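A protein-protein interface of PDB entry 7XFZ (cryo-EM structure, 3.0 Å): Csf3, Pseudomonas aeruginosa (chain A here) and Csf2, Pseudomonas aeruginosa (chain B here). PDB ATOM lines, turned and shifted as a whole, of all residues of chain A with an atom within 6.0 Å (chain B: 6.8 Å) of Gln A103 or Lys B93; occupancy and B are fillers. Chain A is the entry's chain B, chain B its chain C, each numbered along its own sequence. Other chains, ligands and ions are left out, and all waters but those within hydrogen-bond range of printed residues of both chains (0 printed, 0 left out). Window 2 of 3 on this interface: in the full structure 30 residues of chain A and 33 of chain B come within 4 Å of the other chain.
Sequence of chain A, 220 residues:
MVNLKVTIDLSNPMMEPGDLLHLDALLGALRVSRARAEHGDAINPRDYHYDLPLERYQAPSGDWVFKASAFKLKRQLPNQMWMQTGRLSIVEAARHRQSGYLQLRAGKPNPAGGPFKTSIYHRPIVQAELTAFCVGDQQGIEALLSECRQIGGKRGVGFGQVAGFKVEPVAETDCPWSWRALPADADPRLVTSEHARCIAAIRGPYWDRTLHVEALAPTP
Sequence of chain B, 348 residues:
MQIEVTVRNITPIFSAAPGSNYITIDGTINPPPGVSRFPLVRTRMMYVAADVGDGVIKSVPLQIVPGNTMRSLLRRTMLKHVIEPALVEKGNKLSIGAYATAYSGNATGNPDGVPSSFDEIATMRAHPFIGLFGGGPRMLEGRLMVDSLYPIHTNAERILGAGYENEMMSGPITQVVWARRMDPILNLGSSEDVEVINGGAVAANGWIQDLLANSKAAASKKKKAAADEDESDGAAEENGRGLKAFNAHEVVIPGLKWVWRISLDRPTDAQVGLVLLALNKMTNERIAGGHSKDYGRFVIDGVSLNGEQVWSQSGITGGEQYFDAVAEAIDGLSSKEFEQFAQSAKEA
N of Gln A103 is in hydrogen-bond range of O of Leu B94, 2.9 Å away. O of Tyr A101 is in hydrogen-bond range of N of Leu B94, at 3.0 Å.
Along chain A the printed residues that touch a printed residue of chain B span positions 100 to 103. Among the printed residues, no Asp or Glu carboxylate lies within 4 Å of a Lys or Arg side-chain nitrogen of the other chain.
Of the printed residues of chain B, Gly A100 touches Lys B93. Of chain B, only Lys B93 (3.5 Å) and Leu B94 (2.9 Å) come within 4 Å of Gln A103. Of chain A, only Gly A100, Tyr A101 and Gln A103 come within 4 Å of Lys B93. Gly B97 touches none of the printed residues of chain A. Printed residues of chain A within 4 Å of Tyr B99: Leu A102 (3.7 Å). The nearest residue of chain B that does not touch Gln A103 is Ile B96 (4.1 Å). The nearest residue of chain A that does not touch Lys B93 is Leu A102 (5.6 Å). The nearest printed residue of chain A that does not touch Tyr B99 is Tyr A101 (4.2 Å).
O of Lys B93 sits at hydrogen-bond distance from OG of Ser B335, at 2.9 Å. The side-chain amide oxygen (OE1) of Gln A103 lies close to the backbone carbonyl oxygen (O) of Gly A100 (2.9 Å). O of Leu B87 lies within hydrogen-bond range of N of Asn B92 (3.3 Å).
Among the printed residues, merely in contact across the chains: Gly A100 with Lys B93, Gln A103 with Lys B93, Leu A102 with Leu B94, Tyr A101 with Lys B93, Leu A102 with Tyr B99, Tyr A101 with Leu B87 and Tyr A101 with Asn B92.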
ATOM      1  N   ARG A  97     -17.681 -25.795  28.314  1.00  0.00           N
ATOM      2  CA  ARG A  97     -17.236 -27.163  28.073  1.00  0.00           C
ATOM      3  C   ARG A  97     -18.071 -27.829  26.990  1.00  0.00           C
ATOM      4  O   ARG A  97     -17.549 -28.603  26.180  1.00  0.00           O
ATOM      5  CB  ARG A  97     -17.303 -27.961  29.372  1.00  0.00           C
ATOM      6  CG  ARG A  97     -16.815 -29.388  29.271  1.00  0.00           C
ATOM      7  CD  ARG A  97     -17.171 -30.156  30.530  1.00  0.00           C
ATOM      8  NE  ARG A  97     -16.732 -31.543  30.481  1.00  0.00           N
ATOM      9  CZ  ARG A  97     -17.531 -32.571  30.233  1.00  0.00           C
ATOM     10  NH1 ARG A  97     -18.818 -32.399  29.983  1.00  0.00           N
ATOM     11  NH2 ARG A  97     -17.027 -33.800  30.234  1.00  0.00           N
ATOM     12  N   GLY A 100     -16.988 -26.461  23.522  1.00  0.00           N
ATOM     13  CA  GLY A 100     -15.617 -26.701  23.123  1.00  0.00           C
ATOM     14  C   GLY A 100     -14.652 -25.573  23.415  1.00  0.00           C
ATOM     15  O   GLY A 100     -13.455 -25.721  23.142  1.00  0.00           O
ATOM     16  N   TYR A 101     -15.129 -24.453  23.959  1.00  0.00           N
ATOM     17  CA  TYR A 101     -14.250 -23.329  24.263  1.00  0.00           C
ATOM     18  C   TYR A 101     -13.336 -23.634  25.442  1.00  0.00           C
ATOM     19  O   TYR A 101     -12.224 -23.102  25.515  1.00  0.00           O
ATOM     20  CB  TYR A 101     -15.092 -22.082  24.531  1.00  0.00           C
ATOM     21  CG  TYR A 101     -14.344 -20.906  25.115  1.00  0.00           C
ATOM     22  CD1 TYR A 101     -13.471 -20.158  24.341  1.00  0.00           C
ATOM     23  CD2 TYR A 101     -14.530 -20.531  26.436  1.00  0.00           C
ATOM     24  CE1 TYR A 101     -12.795 -19.080  24.871  1.00  0.00           C
ATOM     25  CE2 TYR A 101     -13.858 -19.457  26.975  1.00  0.00           C
ATOM     26  CZ  TYR A 101     -12.994 -18.734  26.189  1.00  0.00           C
ATOM     27  OH  TYR A 101     -12.324 -17.659  26.724  1.00  0.00           O
ATOM     28  N   LEU A 102     -13.781 -24.479  26.366  1.00  0.00           N
ATOM     29  CA  LEU A 102     -12.982 -24.908  27.505  1.00  0.00           C
ATOM     30  C   LEU A 102     -12.629 -26.378  27.331  1.00  0.00           C
ATOM     31  O   LEU A 102     -13.503 -27.200  27.039  1.00  0.00           O
ATOM     32  CB  LEU A 102     -13.737 -24.687  28.817  1.00  0.00           C
ATOM     33  CG  LEU A 102     -13.285 -25.495  30.033  1.00  0.00           C
ATOM     34  CD1 LEU A 102     -11.921 -25.039  30.502  1.00  0.00           C
ATOM     35  CD2 LEU A 102     -14.296 -25.382  31.152  1.00  0.00           C
ATOM     36  N   GLN A 103     -11.348 -26.704  27.501  1.00  0.00           N
ATOM     37  CA  GLN A 103     -10.850 -28.058  27.271  1.00  0.00           C
ATOM     38  C   GLN A 103     -10.749 -28.784  28.610  1.00  0.00           C
ATOM     39  O   GLN A 103      -9.691 -28.865  29.231  1.00  0.00           O
ATOM     40  CB  GLN A 103      -9.509 -28.014  26.548  1.00  0.00           C
ATOM     41  CG  GLN A 103      -9.590 -27.474  25.133  1.00  0.00           C
ATOM     42  CD  GLN A 103     -10.483 -28.314  24.245  1.00  0.00           C
ATOM     43  OE1 GLN A 103     -11.446 -27.817  23.664  1.00  0.00           O
ATOM     44  NE2 GLN A 103     -10.165 -29.598  24.133  1.00  0.00           N
ATOM     45  N   LEU A 104     -11.880 -29.326  29.052  1.00  0.00           N
ATOM     46  CA  LEU A 104     -11.965 -30.065  30.303  1.00  0.00           C
ATOM     47  C   LEU A 104     -12.552 -31.442  30.037  1.00  0.00           C
ATOM     48  O   LEU A 104     -13.565 -31.565  29.343  1.00  0.00           O
ATOM     49  CB  LEU A 104     -12.817 -29.317  31.332  1.00  0.00           C
ATOM     50  CG  LEU A 104     -12.871 -29.941  32.725  1.00  0.00           C
ATOM     51  CD1 LEU A 104     -11.473 -30.242  33.225  1.00  0.00           C
ATOM     52  CD2 LEU A 104     -13.596 -29.023  33.687  1.00  0.00           C
ATOM     53  N   ARG A 105     -11.916 -32.471  30.591  1.00  0.00           N
ATOM     54  CA  ARG A 105     -12.354 -33.848  30.416  1.00  0.00           C
ATOM     55  C   ARG A 105     -12.929 -34.452  31.690  1.00  0.00           C
ATOM     56  O   ARG A 105     -13.425 -35.583  31.655  1.00  0.00           O
ATOM     57  CB  ARG A 105     -11.188 -34.703  29.908  1.00  0.00           C
ATOM     58  CG  ARG A 105     -11.601 -35.868  29.029  1.00  0.00           C
ATOM     59  CD  ARG A 105     -11.164 -37.191  29.634  1.00  0.00           C
ATOM     60  NE  ARG A 105      -9.747 -37.186  29.978  1.00  0.00           N
ATOM     61  CZ  ARG A 105      -8.762 -37.308  29.100  1.00  0.00           C
ATOM     62  NH1 ARG A 105      -9.002 -37.460  27.807  1.00  0.00           N
ATOM     63  NH2 ARG A 105      -7.503 -37.281  29.527  1.00  0.00           N
ATOM     64  N   LEU B  87     -12.158 -14.119  21.032  1.00  0.00           N
ATOM     65  CA  LEU B  87     -11.373 -15.345  21.057  1.00  0.00           C
ATOM     66  C   LEU B  87     -12.059 -16.473  20.301  1.00  0.00           C
ATOM     67  O   LEU B  87     -11.381 -17.289  19.669  1.00  0.00           O
ATOM     68  CB  LEU B  87     -11.108 -15.760  22.504  1.00  0.00           C
ATOM     69  CG  LEU B  87      -9.713 -16.302  22.809  1.00  0.00           C
ATOM     70  CD1 LEU B  87      -8.671 -15.255  22.479  1.00  0.00           C
ATOM     71  CD2 LEU B  87      -9.608 -16.712  24.262  1.00  0.00           C
ATOM     72  N   GLY B  91     -11.308 -19.125  16.574  1.00  0.00           N
ATOM     73  CA  GLY B  91     -11.260 -20.555  16.820  1.00  0.00           C
ATOM     74  C   GLY B  91     -10.251 -20.975  17.867  1.00  0.00           C
ATOM     75  O   GLY B  91      -9.544 -21.973  17.674  1.00  0.00           O
ATOM     76  N   ASN B  92     -10.168 -20.243  18.973  1.00  0.00           N
ATOM     77  CA  ASN B  92      -9.219 -20.528  20.038  1.00  0.00           C
ATOM     78  C   ASN B  92      -9.893 -21.286  21.176  1.00  0.00           C
ATOM     79  O   ASN B  92     -11.115 -21.255  21.342  1.00  0.00           O
ATOM     80  CB  ASN B  92      -8.597 -19.234  20.568  1.00  0.00           C
ATOM     81  CG  ASN B  92      -7.583 -18.645  19.613  1.00  0.00           C
ATOM     82  OD1 ASN B  92      -7.730 -17.514  19.157  1.00  0.00           O
ATOM     83  ND2 ASN B  92      -6.547 -19.411  19.303  1.00  0.00           N
ATOM     84  N   LYS B  93      -9.068 -21.972  21.965  1.00  0.00           N
ATOM     85  CA  LYS B  93      -9.529 -22.779  23.083  1.00  0.00           C
ATOM     86  C   LYS B  93      -8.647 -22.522  24.296  1.00  0.00           C
ATOM     87  O   LYS B  93      -7.503 -22.081  24.168  1.00  0.00           O
ATOM     88  CB  LYS B  93      -9.515 -24.271  22.740  1.00  0.00           C
ATOM     89  CG  LYS B  93     -10.562 -24.676  21.723  1.00  0.00           C
ATOM     90  CD  LYS B  93     -10.182 -25.972  21.033  1.00  0.00           C
ATOM     91  CE  LYS B  93     -11.247 -26.385  20.036  1.00  0.00           C
ATOM     92  NZ  LYS B  93     -11.585 -25.272  19.111  1.00  0.00           N
ATOM     93  N   LEU B  94      -9.190 -22.800  25.476  1.00  0.00           N
ATOM     94  CA  LEU B  94      -8.498 -22.572  26.737  1.00  0.00           C
ATOM     95  C   LEU B  94      -8.400 -23.876  27.514  1.00  0.00           C
ATOM     96  O   LEU B  94      -9.377 -24.627  27.597  1.00  0.00           O
ATOM     97  CB  LEU B  94      -9.223 -21.516  27.572  1.00  0.00           C
ATOM     98  CG  LEU B  94      -8.982 -20.047  27.224  1.00  0.00           C
ATOM     99  CD1 LEU B  94      -9.665 -19.144  28.232  1.00  0.00           C
ATOM    100  CD2 LEU B  94      -7.496 -19.748  27.164  1.00  0.00           C
ATOM    101  N   SER B  95      -7.227 -24.145  28.075  1.00  0.00           N
ATOM    102  CA  SER B  95      -7.077 -25.257  28.995  1.00  0.00           C
ATOM    103  C   SER B  95      -7.709 -24.904  30.338  1.00  0.00           C
ATOM    104  O   SER B  95      -8.127 -23.769  30.578  1.00  0.00           O
ATOM    105  CB  SER B  95      -5.603 -25.617  29.168  1.00  0.00           C
ATOM    106  OG  SER B  95      -4.859 -24.508  29.635  1.00  0.00           O
ATOM    107  N   ILE B  96      -7.786 -25.894  31.226  1.00  0.00           N
ATOM    108  CA  ILE B  96      -8.438 -25.658  32.512  1.00  0.00           C
ATOM    109  C   ILE B  96      -7.626 -24.683  33.356  1.00  0.00           C
ATOM    110  O   ILE B  96      -8.187 -23.836  34.059  1.00  0.00           O
ATOM    111  CB  ILE B  96      -8.695 -26.989  33.245  1.00  0.00           C
ATOM    112  CG1 ILE B  96      -9.494 -26.743  34.528  1.00  0.00           C
ATOM    113  CG2 ILE B  96      -7.395 -27.725  33.531  1.00  0.00           C
ATOM    114  CD1 ILE B  96     -10.752 -25.923  34.320  1.00  0.00           C
ATOM    115  N   GLY B  97      -6.296 -24.773  33.295  1.00  0.00           N
ATOM    116  CA  GLY B  97      -5.471 -23.839  34.048  1.00  0.00           C
ATOM    117  C   GLY B  97      -5.611 -22.407  33.566  1.00  0.00           C
ATOM    118  O   GLY B  97      -5.796 -21.487  34.368  1.00  0.00           O
ATOM    119  N   ALA B  98      -5.540 -22.201  32.249  1.00  0.00           N
ATOM    120  CA  ALA B  98      -5.694 -20.860  31.697  1.00  0.00           C
ATOM    121  C   ALA B  98      -7.095 -20.319  31.947  1.00  0.00           C
ATOM    122  O   ALA B  98      -7.265 -19.140  32.273  1.00  0.00           O
ATOM    123  CB  ALA B  98      -5.381 -20.868  30.203  1.00  0.00           C
ATOM    124  N   TYR B  99      -8.109 -21.172  31.795  1.00  0.00           N
ATOM    125  CA  TYR B  99      -9.485 -20.756  32.046  1.00  0.00           C
ATOM    126  C   TYR B  99      -9.674 -20.328  33.497  1.00  0.00           C
ATOM    127  O   TYR B  99     -10.253 -19.272  33.773  1.00  0.00           O
ATOM    128  CB  TYR B  99     -10.433 -21.900  31.685  1.00  0.00           C
ATOM    129  CG  TYR B  99     -11.901 -21.605  31.865  1.00  0.00           C
ATOM    130  CD1 TYR B  99     -12.643 -21.042  30.841  1.00  0.00           C
ATOM    131  CD2 TYR B  99     -12.551 -21.913  33.051  1.00  0.00           C
ATOM    132  CE1 TYR B  99     -13.984 -20.780  30.996  1.00  0.00           C
ATOM    133  CE2 TYR B  99     -13.892 -21.651  33.214  1.00  0.00           C
ATOM    134  CZ  TYR B  99     -14.602 -21.086  32.184  1.00  0.00           C
ATOM    135  OH  TYR B  99     -15.940 -20.823  32.339  1.00  0.00           O
ATOM    136  N   SER B 335      -4.917 -17.264  22.421  1.00  0.00           N
ATOM    137  CA  SER B 335      -4.860 -18.050  23.643  1.00  0.00           C
ATOM    138  C   SER B 335      -3.435 -18.294  24.120  1.00  0.00           C
ATOM    139  O   SER B 335      -3.247 -18.695  25.271  1.00  0.00           O
ATOM    140  CB  SER B 335      -5.570 -19.387  23.432  1.00  0.00           C
ATOM    141  OG  SER B 335      -5.173 -20.338  24.402  1.00  0.00           O
ATOM    142  N   LYS B 336      -2.434 -18.054  23.269  1.00  0.00           N
ATOM    143  CA  LYS B 336      -1.051 -18.351  23.634  1.00  0.00           C
ATOM    144  C   LYS B 336      -0.581 -17.496  24.806  1.00  0.00           C
ATOM    145  O   LYS B 336       0.130 -17.985  25.691  1.00  0.00           O
ATOM    146  CB  LYS B 336      -0.146 -18.158  22.418  1.00  0.00           C
ATOM    147  CG  LYS B 336       1.338 -18.170  22.724  1.00  0.00           C
ATOM    148  CD  LYS B 336       1.965 -16.824  22.411  1.00  0.00           C
ATOM    149  CE  LYS B 336       3.001 -16.438  23.448  1.00  0.00           C
ATOM    150  NZ  LYS B 336       3.627 -15.121  23.145  1.00  0.00           N
ATOM    151  N   GLU B 339      -2.059 -18.983  27.912  1.00  0.00           N
ATOM    152  CA  GLU B 339      -1.357 -20.202  28.304  1.00  0.00           C
ATOM    153  C   GLU B 339      -0.004 -19.887  28.928  1.00  0.00           C
ATOM    154  O   GLU B 339       0.426 -20.564  29.867  1.00  0.00           O
ATOM    155  CB  GLU B 339      -1.183 -21.127  27.101  1.00  0.00           C
ATOM    156  CG  GLU B 339      -2.462 -21.443  26.348  1.00  0.00           C
ATOM    157  CD  GLU B 339      -3.437 -22.265  27.159  1.00  0.00           C
ATOM    158  OE1 GLU B 339      -2.998 -23.211  27.843  1.00  0.00           O
ATOM    159  OE2 GLU B 339      -4.647 -21.967  27.111  1.00  0.00           O
